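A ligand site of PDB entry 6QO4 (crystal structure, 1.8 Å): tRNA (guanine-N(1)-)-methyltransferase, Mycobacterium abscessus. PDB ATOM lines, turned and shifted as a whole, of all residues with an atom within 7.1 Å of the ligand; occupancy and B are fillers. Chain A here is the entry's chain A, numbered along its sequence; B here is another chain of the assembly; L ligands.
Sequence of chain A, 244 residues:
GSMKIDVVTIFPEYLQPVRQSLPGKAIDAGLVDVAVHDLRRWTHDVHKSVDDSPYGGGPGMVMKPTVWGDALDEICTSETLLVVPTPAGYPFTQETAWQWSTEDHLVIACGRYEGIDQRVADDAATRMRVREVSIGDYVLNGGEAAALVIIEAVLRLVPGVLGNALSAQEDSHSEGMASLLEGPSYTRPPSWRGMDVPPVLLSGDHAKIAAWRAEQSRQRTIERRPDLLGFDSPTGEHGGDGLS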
ATOM      1  N   VAL A  84       4.923  21.539 -19.533  1.00  0.00           N
ATOM      2  CA  VAL A  84       5.930  22.547 -19.792  1.00  0.00           C
ATOM      3  C   VAL A  84       5.716  23.101 -21.180  1.00  0.00           C
ATOM      4  O   VAL A  84       6.069  22.462 -22.168  1.00  0.00           O
ATOM      5  CB  VAL A  84       7.373  21.976 -19.704  1.00  0.00           C
ATOM      6  CG1 VAL A  84       8.418  23.081 -19.900  1.00  0.00           C
ATOM      7  CG2 VAL A  84       7.608  21.263 -18.362  1.00  0.00           C
ATOM      8  N   PRO A  85       5.122  24.291 -21.264  1.00  0.00           N
ATOM      9  CA  PRO A  85       5.015  24.887 -22.605  1.00  0.00           C
ATOM     10  C   PRO A  85       6.393  25.222 -23.179  1.00  0.00           C
ATOM     11  O   PRO A  85       7.308  25.699 -22.492  1.00  0.00           O
ATOM     12  CB  PRO A  85       4.164  26.145 -22.371  1.00  0.00           C
ATOM     13  CG  PRO A  85       3.386  25.842 -21.107  1.00  0.00           C
ATOM     14  CD  PRO A  85       4.344  25.041 -20.266  1.00  0.00           C
ATOM     15  N   THR A  86       6.554  24.924 -24.451  1.00  0.00           N
ATOM     16  CA  THR A  86       7.804  25.195 -25.139  1.00  0.00           C
ATOM     17  C   THR A  86       7.565  25.176 -26.624  1.00  0.00           C
ATOM     18  O   THR A  86       6.760  24.379 -27.111  1.00  0.00           O
ATOM     19  CB  THR A  86       8.902  24.165 -24.753  1.00  0.00           C
ATOM     20  OG1 THR A  86       9.952  24.232 -25.732  1.00  0.00           O
ATOM     21  CG2 THR A  86       8.350  22.770 -24.674  1.00  0.00           C
ATOM     22  N   PRO A  87       8.259  26.057 -27.354  1.00  0.00           N
ATOM     23  CA  PRO A  87       8.157  26.078 -28.820  1.00  0.00           C
ATOM     24  C   PRO A  87       8.627  24.780 -29.446  1.00  0.00           C
ATOM     25  O   PRO A  87       8.252  24.472 -30.570  1.00  0.00           O
ATOM     26  CB  PRO A  87       9.097  27.232 -29.238  1.00  0.00           C
ATOM     27  CG  PRO A  87       9.393  27.968 -27.992  1.00  0.00           C
ATOM     28  CD  PRO A  87       9.256  27.016 -26.850  1.00  0.00           C
ATOM     29  N   ALA A  88       9.450  24.021 -28.717  1.00  0.00           N
ATOM     30  CA  ALA A  88       9.938  22.734 -29.204  1.00  0.00           C
ATOM     31  C   ALA A  88       9.128  21.538 -28.694  1.00  0.00           C
ATOM     32  O   ALA A  88       9.603  20.405 -28.704  1.00  0.00           O
ATOM     33  CB  ALA A  88      11.416  22.565 -28.805  1.00  0.00           C
ATOM     34  N   GLY A  89       7.906  21.793 -28.238  1.00  0.00           N
ATOM     35  CA  GLY A  89       7.091  20.736 -27.665  1.00  0.00           C
ATOM     36  C   GLY A  89       6.334  19.900 -28.688  1.00  0.00           C
ATOM     37  O   GLY A  89       6.294  20.235 -29.881  1.00  0.00           O
ATOM     38  N   ALA A 109       4.627  24.792 -15.801  1.00  0.00           N
ATOM     39  CA  ALA A 109       5.875  25.519 -15.594  1.00  0.00           C
ATOM     40  C   ALA A 109       6.120  26.479 -16.741  1.00  0.00           C
ATOM     41  O   ALA A 109       6.449  26.070 -17.868  1.00  0.00           O
ATOM     42  CB  ALA A 109       7.027  24.533 -15.447  1.00  0.00           C
ATOM     43  N   CYS A 110       5.955  27.782 -16.464  1.00  0.00           N
ATOM     44  CA  CYS A 110       6.108  28.817 -17.487  1.00  0.00           C
ATOM     45  C   CYS A 110       7.522  29.340 -17.545  1.00  0.00           C
ATOM     46  O   CYS A 110       8.031  29.900 -16.566  1.00  0.00           O
ATOM     47  CB  CYS A 110       5.152  29.995 -17.218  1.00  0.00           C
ATOM     48  SG  CYS A 110       3.415  29.511 -17.134  1.00  0.00           S
ATOM     49  N   GLY A 111       8.164  29.177 -18.685  1.00  0.00           N
ATOM     50  CA  GLY A 111       9.545  29.606 -18.848  1.00  0.00           C
ATOM     51  C   GLY A 111       9.657  30.590 -19.984  1.00  0.00           C
ATOM     52  O   GLY A 111       8.696  30.800 -20.712  1.00  0.00           O
ATOM     53  N   ARG A 112      10.829  31.182 -20.150  1.00  0.00           N
ATOM     54  CA  ARG A 112      11.059  32.096 -21.263  1.00  0.00           C
ATOM     55  C   ARG A 112      11.359  31.310 -22.537  1.00  0.00           C
ATOM     56  O   ARG A 112      11.610  30.100 -22.484  1.00  0.00           O
ATOM     57  CB  ARG A 112      12.198  33.060 -20.937  1.00  0.00           C
ATOM     58  CG  ARG A 112      13.473  32.360 -20.490  1.00  0.00           C
ATOM     59  CD  ARG A 112      14.536  33.382 -20.074  1.00  0.00           C
ATOM     60  NE  ARG A 112      14.944  34.200 -21.209  1.00  0.00           N
ATOM     61  CZ  ARG A 112      15.507  35.405 -21.115  1.00  0.00           C
ATOM     62  NH1 ARG A 112      15.847  36.069 -22.203  1.00  0.00           N
ATOM     63  NH2 ARG A 112      15.717  35.944 -19.921  1.00  0.00           N
ATOM     64  N   TYR A 113      11.338  32.003 -23.673  1.00  0.00           N
ATOM     65  CA  TYR A 113      11.528  31.367 -24.972  1.00  0.00           C
ATOM     66  C   TYR A 113      12.811  30.530 -25.072  1.00  0.00           C
ATOM     67  O   TYR A 113      12.800  29.432 -25.625  1.00  0.00           O
ATOM     68  CB  TYR A 113      11.536  32.428 -26.094  1.00  0.00           C
ATOM     69  CG  TYR A 113      11.893  31.838 -27.433  1.00  0.00           C
ATOM     70  CD1 TYR A 113      10.994  31.005 -28.093  1.00  0.00           C
ATOM     71  CD2 TYR A 113      13.126  32.090 -28.024  1.00  0.00           C
ATOM     72  CE1 TYR A 113      11.312  30.449 -29.331  1.00  0.00           C
ATOM     73  CE2 TYR A 113      13.446  31.534 -29.252  1.00  0.00           C
ATOM     74  CZ  TYR A 113      12.533  30.712 -29.899  1.00  0.00           C
ATOM     75  OH  TYR A 113      12.834  30.146 -31.122  1.00  0.00           O
ATOM     76  N   GLU A 114      13.913  31.045 -24.532  1.00  0.00           N
ATOM     77  CA  GLU A 114      15.197  30.350 -24.601  1.00  0.00           C
ATOM     78  C   GLU A 114      15.216  29.053 -23.794  1.00  0.00           C
ATOM     79  O   GLU A 114      16.037  28.177 -24.042  1.00  0.00           O
ATOM     80  CB  GLU A 114      16.329  31.258 -24.120  1.00  0.00           C
ATOM     81  CG  GLU A 114      16.622  32.438 -25.021  1.00  0.00           C
ATOM     82  CD  GLU A 114      15.664  33.581 -24.813  1.00  0.00           C
ATOM     83  OE1 GLU A 114      14.883  33.545 -23.826  1.00  0.00           O
ATOM     84  OE2 GLU A 114      15.687  34.534 -25.630  1.00  0.00           O
ATOM     85  N   GLY A 115      14.317  28.950 -22.820  1.00  0.00           N
ATOM     86  CA  GLY A 115      14.040  27.675 -22.190  1.00  0.00           C
ATOM     87  C   GLY A 115      14.486  27.510 -20.754  1.00  0.00           C
ATOM     88  O   GLY A 115      15.226  28.339 -20.210  1.00  0.00           O
ATOM     89  N   VAL A 133       4.935  20.750 -24.429  1.00  0.00           N
ATOM     90  CA  VAL A 133       3.970  20.980 -25.504  1.00  0.00           C
ATOM     91  C   VAL A 133       4.034  22.394 -26.074  1.00  0.00           C
ATOM     92  O   VAL A 133       4.328  23.362 -25.372  1.00  0.00           O
ATOM     93  CB  VAL A 133       2.505  20.714 -25.033  1.00  0.00           C
ATOM     94  CG1 VAL A 133       2.289  19.229 -24.715  1.00  0.00           C
ATOM     95  CG2 VAL A 133       2.159  21.574 -23.819  1.00  0.00           C
ATOM     96  N   SER A 134       3.734  22.489 -27.370  1.00  0.00           N
ATOM     97  CA  SER A 134       3.593  23.772 -28.055  1.00  0.00           C
ATOM     98  C   SER A 134       2.130  24.013 -28.406  1.00  0.00           C
ATOM     99  O   SER A 134       1.391  23.062 -28.714  1.00  0.00           O
ATOM    100  CB  SER A 134       4.464  23.795 -29.320  1.00  0.00           C
ATOM    101  OG  SER A 134       3.913  24.665 -30.289  1.00  0.00           O
ATOM    102  N   ILE A 135       1.687  25.264 -28.372  1.00  0.00           N
ATOM    103  CA  ILE A 135       0.275  25.519 -28.714  1.00  0.00           C
ATOM    104  C   ILE A 135       0.078  26.013 -30.157  1.00  0.00           C
ATOM    105  O   ILE A 135      -1.059  26.239 -30.596  1.00  0.00           O
ATOM    106  CB  ILE A 135      -0.382  26.537 -27.745  1.00  0.00           C
ATOM    107  CG1 ILE A 135       0.378  27.867 -27.761  1.00  0.00           C
ATOM    108  CG2 ILE A 135      -0.449  25.957 -26.322  1.00  0.00           C
ATOM    109  CD1 ILE A 135      -0.479  29.050 -27.258  1.00  0.00           C
ATOM    110  N   GLY A 136       1.174  26.150 -30.901  1.00  0.00           N
ATOM    111  CA  GLY A 136       1.084  26.563 -32.287  1.00  0.00           C
ATOM    112  C   GLY A 136       2.432  26.944 -32.865  1.00  0.00           C
ATOM    113  O   GLY A 136       3.429  26.968 -32.146  1.00  0.00           O
ATOM    114  N   ASP A 137       2.475  27.266 -34.149  1.00  0.00           N
ATOM    115  CA  ASP A 137       3.737  27.587 -34.788  1.00  0.00           C
ATOM    116  C   ASP A 137       3.904  29.094 -34.899  1.00  0.00           C
ATOM    117  O   ASP A 137       3.838  29.679 -35.983  1.00  0.00           O
ATOM    118  CB  ASP A 137       3.838  26.941 -36.159  1.00  0.00           C
ATOM    119  CG  ASP A 137       4.001  25.439 -36.076  1.00  0.00           C
ATOM    120  OD1 ASP A 137       4.733  24.976 -35.171  1.00  0.00           O
ATOM    121  OD2 ASP A 137       3.382  24.737 -36.895  1.00  0.00           O
ATOM    122  N   TYR A 138       4.115  29.699 -33.757  1.00  0.00           N
ATOM    123  CA  TYR A 138       4.451  31.108 -33.651  1.00  0.00           C
ATOM    124  C   TYR A 138       5.297  31.170 -32.402  1.00  0.00           C
ATOM    125  O   TYR A 138       5.298  30.235 -31.591  1.00  0.00           O
ATOM    126  CB  TYR A 138       3.197  31.985 -33.558  1.00  0.00           C
ATOM    127  CG  TYR A 138       2.079  31.316 -32.809  1.00  0.00           C
ATOM    128  CD1 TYR A 138       2.080  31.254 -31.422  1.00  0.00           C
ATOM    129  CD2 TYR A 138       1.014  30.724 -33.492  1.00  0.00           C
ATOM    130  CE1 TYR A 138       1.060  30.629 -30.727  1.00  0.00           C
ATOM    131  CE2 TYR A 138      -0.022  30.097 -32.804  1.00  0.00           C
ATOM    132  CZ  TYR A 138       0.010  30.062 -31.424  1.00  0.00           C
ATOM    133  OH  TYR A 138      -0.996  29.439 -30.733  1.00  0.00           O
ATOM    134  N   VAL A 139       6.007  32.279 -32.242  1.00  0.00           N
ATOM    135  CA  VAL A 139       6.920  32.420 -31.122  1.00  0.00           C
ATOM    136  C   VAL A 139       6.363  33.422 -30.116  1.00  0.00           C
ATOM    137  O   VAL A 139       6.084  34.565 -30.450  1.00  0.00           O
ATOM    138  CB  VAL A 139       8.300  32.873 -31.584  1.00  0.00           C
ATOM    139  CG1 VAL A 139       9.233  33.050 -30.387  1.00  0.00           C
ATOM    140  CG2 VAL A 139       8.878  31.882 -32.585  1.00  0.00           C
ATOM    141  N   LEU A 140       6.194  32.956 -28.894  1.00  0.00           N
ATOM    142  CA  LEU A 140       5.854  33.820 -27.774  1.00  0.00           C
ATOM    143  C   LEU A 140       7.123  34.116 -27.007  1.00  0.00           C
ATOM    144  O   LEU A 140       8.074  33.338 -27.079  1.00  0.00           O
ATOM    145  CB  LEU A 140       4.840  33.159 -26.835  1.00  0.00           C
ATOM    146  CG  LEU A 140       3.576  32.595 -27.470  1.00  0.00           C
ATOM    147  CD1 LEU A 140       2.822  31.726 -26.489  1.00  0.00           C
ATOM    148  CD2 LEU A 140       2.672  33.728 -27.964  1.00  0.00           C
ATOM    149  N   ASN A 141       7.137  35.199 -26.239  1.00  0.00           N
ATOM    150  CA  ASN A 141       8.317  35.503 -25.440  1.00  0.00           C
ATOM    151  C   ASN A 141       8.471  34.590 -24.223  1.00  0.00           C
ATOM    152  O   ASN A 141       9.583  34.393 -23.716  1.00  0.00           O
ATOM    153  CB  ASN A 141       8.289  36.948 -24.990  1.00  0.00           C
ATOM    154  CG  ASN A 141       9.612  37.621 -25.212  1.00  0.00           C
ATOM    155  OD1 ASN A 141      10.073  37.739 -26.349  1.00  0.00           O
ATOM    156  ND2 ASN A 141      10.243  38.073 -24.128  1.00  0.00           N
ATOM    157  N   GLY A 142       7.347  34.065 -23.750  1.00  0.00           N
ATOM    158  CA  GLY A 142       7.351  33.176 -22.590  1.00  0.00           C
ATOM    159  C   GLY A 142       6.131  32.281 -22.568  1.00  0.00           C
ATOM    160  O   GLY A 142       5.225  32.452 -23.370  1.00  0.00           O
ATOM    161  N   GLY A 143       6.104  31.324 -21.647  1.00  0.00           N
ATOM    162  CA  GLY A 143       5.060  30.318 -21.605  1.00  0.00           C
ATOM    163  C   GLY A 143       3.713  30.744 -21.038  1.00  0.00           C
ATOM    164  O   GLY A 143       2.748  29.982 -21.128  1.00  0.00           O
ATOM    165  N   GLU A 144       3.629  31.949 -20.483  1.00  0.00           N
ATOM    166  CA  GLU A 144       2.426  32.406 -19.786  1.00  0.00           C
ATOM    167  C   GLU A 144       1.141  32.368 -20.642  1.00  0.00           C
ATOM    168  O   GLU A 144       0.114  31.816 -20.213  1.00  0.00           O
ATOM    169  CB  GLU A 144       2.633  33.832 -19.258  1.00  0.00           C
ATOM    170  CG  GLU A 144       3.452  33.896 -17.963  1.00  0.00           C
ATOM    171  CD  GLU A 144       4.936  33.692 -18.182  1.00  0.00           C
ATOM    172  OE1 GLU A 144       5.423  33.878 -19.325  1.00  0.00           O
ATOM    173  OE2 GLU A 144       5.642  33.336 -17.199  1.00  0.00           O
ATOM    174  N   ALA A 146       0.646  30.668 -23.331  1.00  0.00           N
ATOM    175  CA  ALA A 146       0.373  29.254 -23.637  1.00  0.00           C
ATOM    176  C   ALA A 146      -0.337  28.585 -22.472  1.00  0.00           C
ATOM    177  O   ALA A 146      -1.255  27.784 -22.665  1.00  0.00           O
ATOM    178  CB  ALA A 146       1.650  28.531 -23.972  1.00  0.00           C
ATOM    179  N   GLU B 152       0.947  39.030 -28.218  1.00  0.00           N
ATOM    180  CA  GLU B 152       2.314  38.745 -27.804  1.00  0.00           C
ATOM    181  C   GLU B 152       3.197  38.338 -28.980  1.00  0.00           C
ATOM    182  O   GLU B 152       4.345  38.774 -29.067  1.00  0.00           O
ATOM    183  CB  GLU B 152       2.344  37.662 -26.722  1.00  0.00           C
ATOM    184  CG  GLU B 152       3.721  37.556 -26.093  1.00  0.00           C
ATOM    185  CD  GLU B 152       3.698  36.906 -24.742  1.00  0.00           C
ATOM    186  OE1 GLU B 152       2.643  36.977 -24.069  1.00  0.00           O
ATOM    187  OE2 GLU B 152       4.736  36.318 -24.362  1.00  0.00           O
ATOM    188  N   ARG B 156       6.383  41.246 -30.250  1.00  0.00           N
ATOM    189  CA  ARG B 156       7.811  40.991 -30.055  1.00  0.00           C
ATOM    190  C   ARG B 156       8.590  41.174 -31.360  1.00  0.00           C
ATOM    191  O   ARG B 156       9.830  41.234 -31.357  1.00  0.00           O
ATOM    192  CB  ARG B 156       8.042  39.602 -29.463  1.00  0.00           C
ATOM    193  CG  ARG B 156       7.610  38.448 -30.306  1.00  0.00           C
ATOM    194  CD  ARG B 156       7.848  37.134 -29.542  1.00  0.00           C
ATOM    195  NE  ARG B 156       9.265  36.897 -29.293  1.00  0.00           N
ATOM    196  CZ  ARG B 156      10.119  36.442 -30.216  1.00  0.00           C
ATOM    197  NH1 ARG B 156       9.708  36.190 -31.454  1.00  0.00           N
ATOM    198  NH2 ARG B 156      11.397  36.254 -29.903  1.00  0.00           N
HETATM  199  O1  LIG L   1       7.296  30.709 -27.585  1.00  0.00           O
HETATM  200  C1  LIG L   1       7.203  30.039 -26.360  1.00  0.00           C
HETATM  201  C2  LIG L   1       8.036  30.436 -25.324  1.00  0.00           C
HETATM  202  C3  LIG L   1       7.975  29.792 -24.098  1.00  0.00           C
HETATM  203  C4  LIG L   1       7.077  28.766 -23.916  1.00  0.00           C
HETATM  204  C5  LIG L   1       6.241  28.362 -24.940  1.00  0.00           C
HETATM  205  C6  LIG L   1       6.293  28.997 -26.175  1.00  0.00           C
HETATM  206  C7  LIG L   1       5.418  28.550 -27.170  1.00  0.00           C
HETATM  207  O2  LIG L   1       4.463  27.616 -26.985  1.00  0.00           O
HETATM  208  N1  LIG L   1       3.785  27.418 -28.170  1.00  0.00           N
HETATM  209  C8  LIG L   1       4.311  28.224 -29.097  1.00  0.00           C
HETATM  210  C9  LIG L   1       5.344  28.950 -28.499  1.00  0.00           C
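The side-chain hydroxyl of Tyr 138 sits at hydrogen-bond distance from the backbone carbonyl oxygen of Ile 135, at 3.2 Å. OG of Ser 134 sits at hydrogen-bond distance from O of Gly 136 (3.0 Å). The backbone NH (N) of Gly 143 is in hydrogen-bond range of the backbone carbonyl oxygen (O) of Gly 111. N of Thr 86 lies within hydrogen-bond range of O of Val 133, 2.9 Å away. OG1 of Thr 86 lies within hydrogen-bond range of N of Ala 88, at 3.0 Å. The backbone NH (N) of Tyr 113 lies within hydrogen-bond range of the backbone carbonyl oxygen (O) of Asn 141, at 3.0 Å. OE1 of Glu 114 is in salt-bridge range of NE of Arg 112, 2.7 Å away.
The backbone NH (N) of Leu 140 is in hydrogen-bond range of an oxygen (O1) of the ligand (2.8 Å). The backbone carbonyl oxygen of Leu 140 sits at hydrogen-bond distance from an oxygen (O1) of the ligand (2.8 Å). N of Ile 135 sits at hydrogen-bond distance from N1 of the ligand (3.0 Å). The side-chain hydroxyl of Ser 134 is in hydrogen-bond range of a nitrogen (N1) of the ligand, 3.5 Å away.
Pro 85 touches the ligand (O to C4, 3.4 Å). Thr 86 touches the ligand. Pro 87 touches the ligand. O of Gly 111 touches C3 of the ligand, 3.6 Å away. O of Arg 112 touches C3 of the ligand, at 3.99 Å. CA of Tyr 113 touches C2 of the ligand, at 3.6 Å. Gly 136 touches the ligand. Tyr 138 touches the ligand (O to C9, 3.3 Å). C of Val 139 touches O1 of the ligand, at 3.8 Å. C of Gly 142 touches C3 of the ligand, at 3.5 Å. Gly 143 touches the ligand (CA to C4, 3.4 Å). Hydrophobic or aromatic side chains that line the ligand: Pro 85, Pro 87, Tyr 113, Ile 135 and Leu 140. Within 4 Å of the ligand: Pro 85, Thr 86, Pro 87, Gly 111, Arg 112, Tyr 113, Ser 134, Ile 135, Gly 136, Tyr 138, Val 139, Leu 140, Gly 142 and Gly 143. The nearest printed residue that does not touch the ligand is Ala 146 (4.2 Å).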
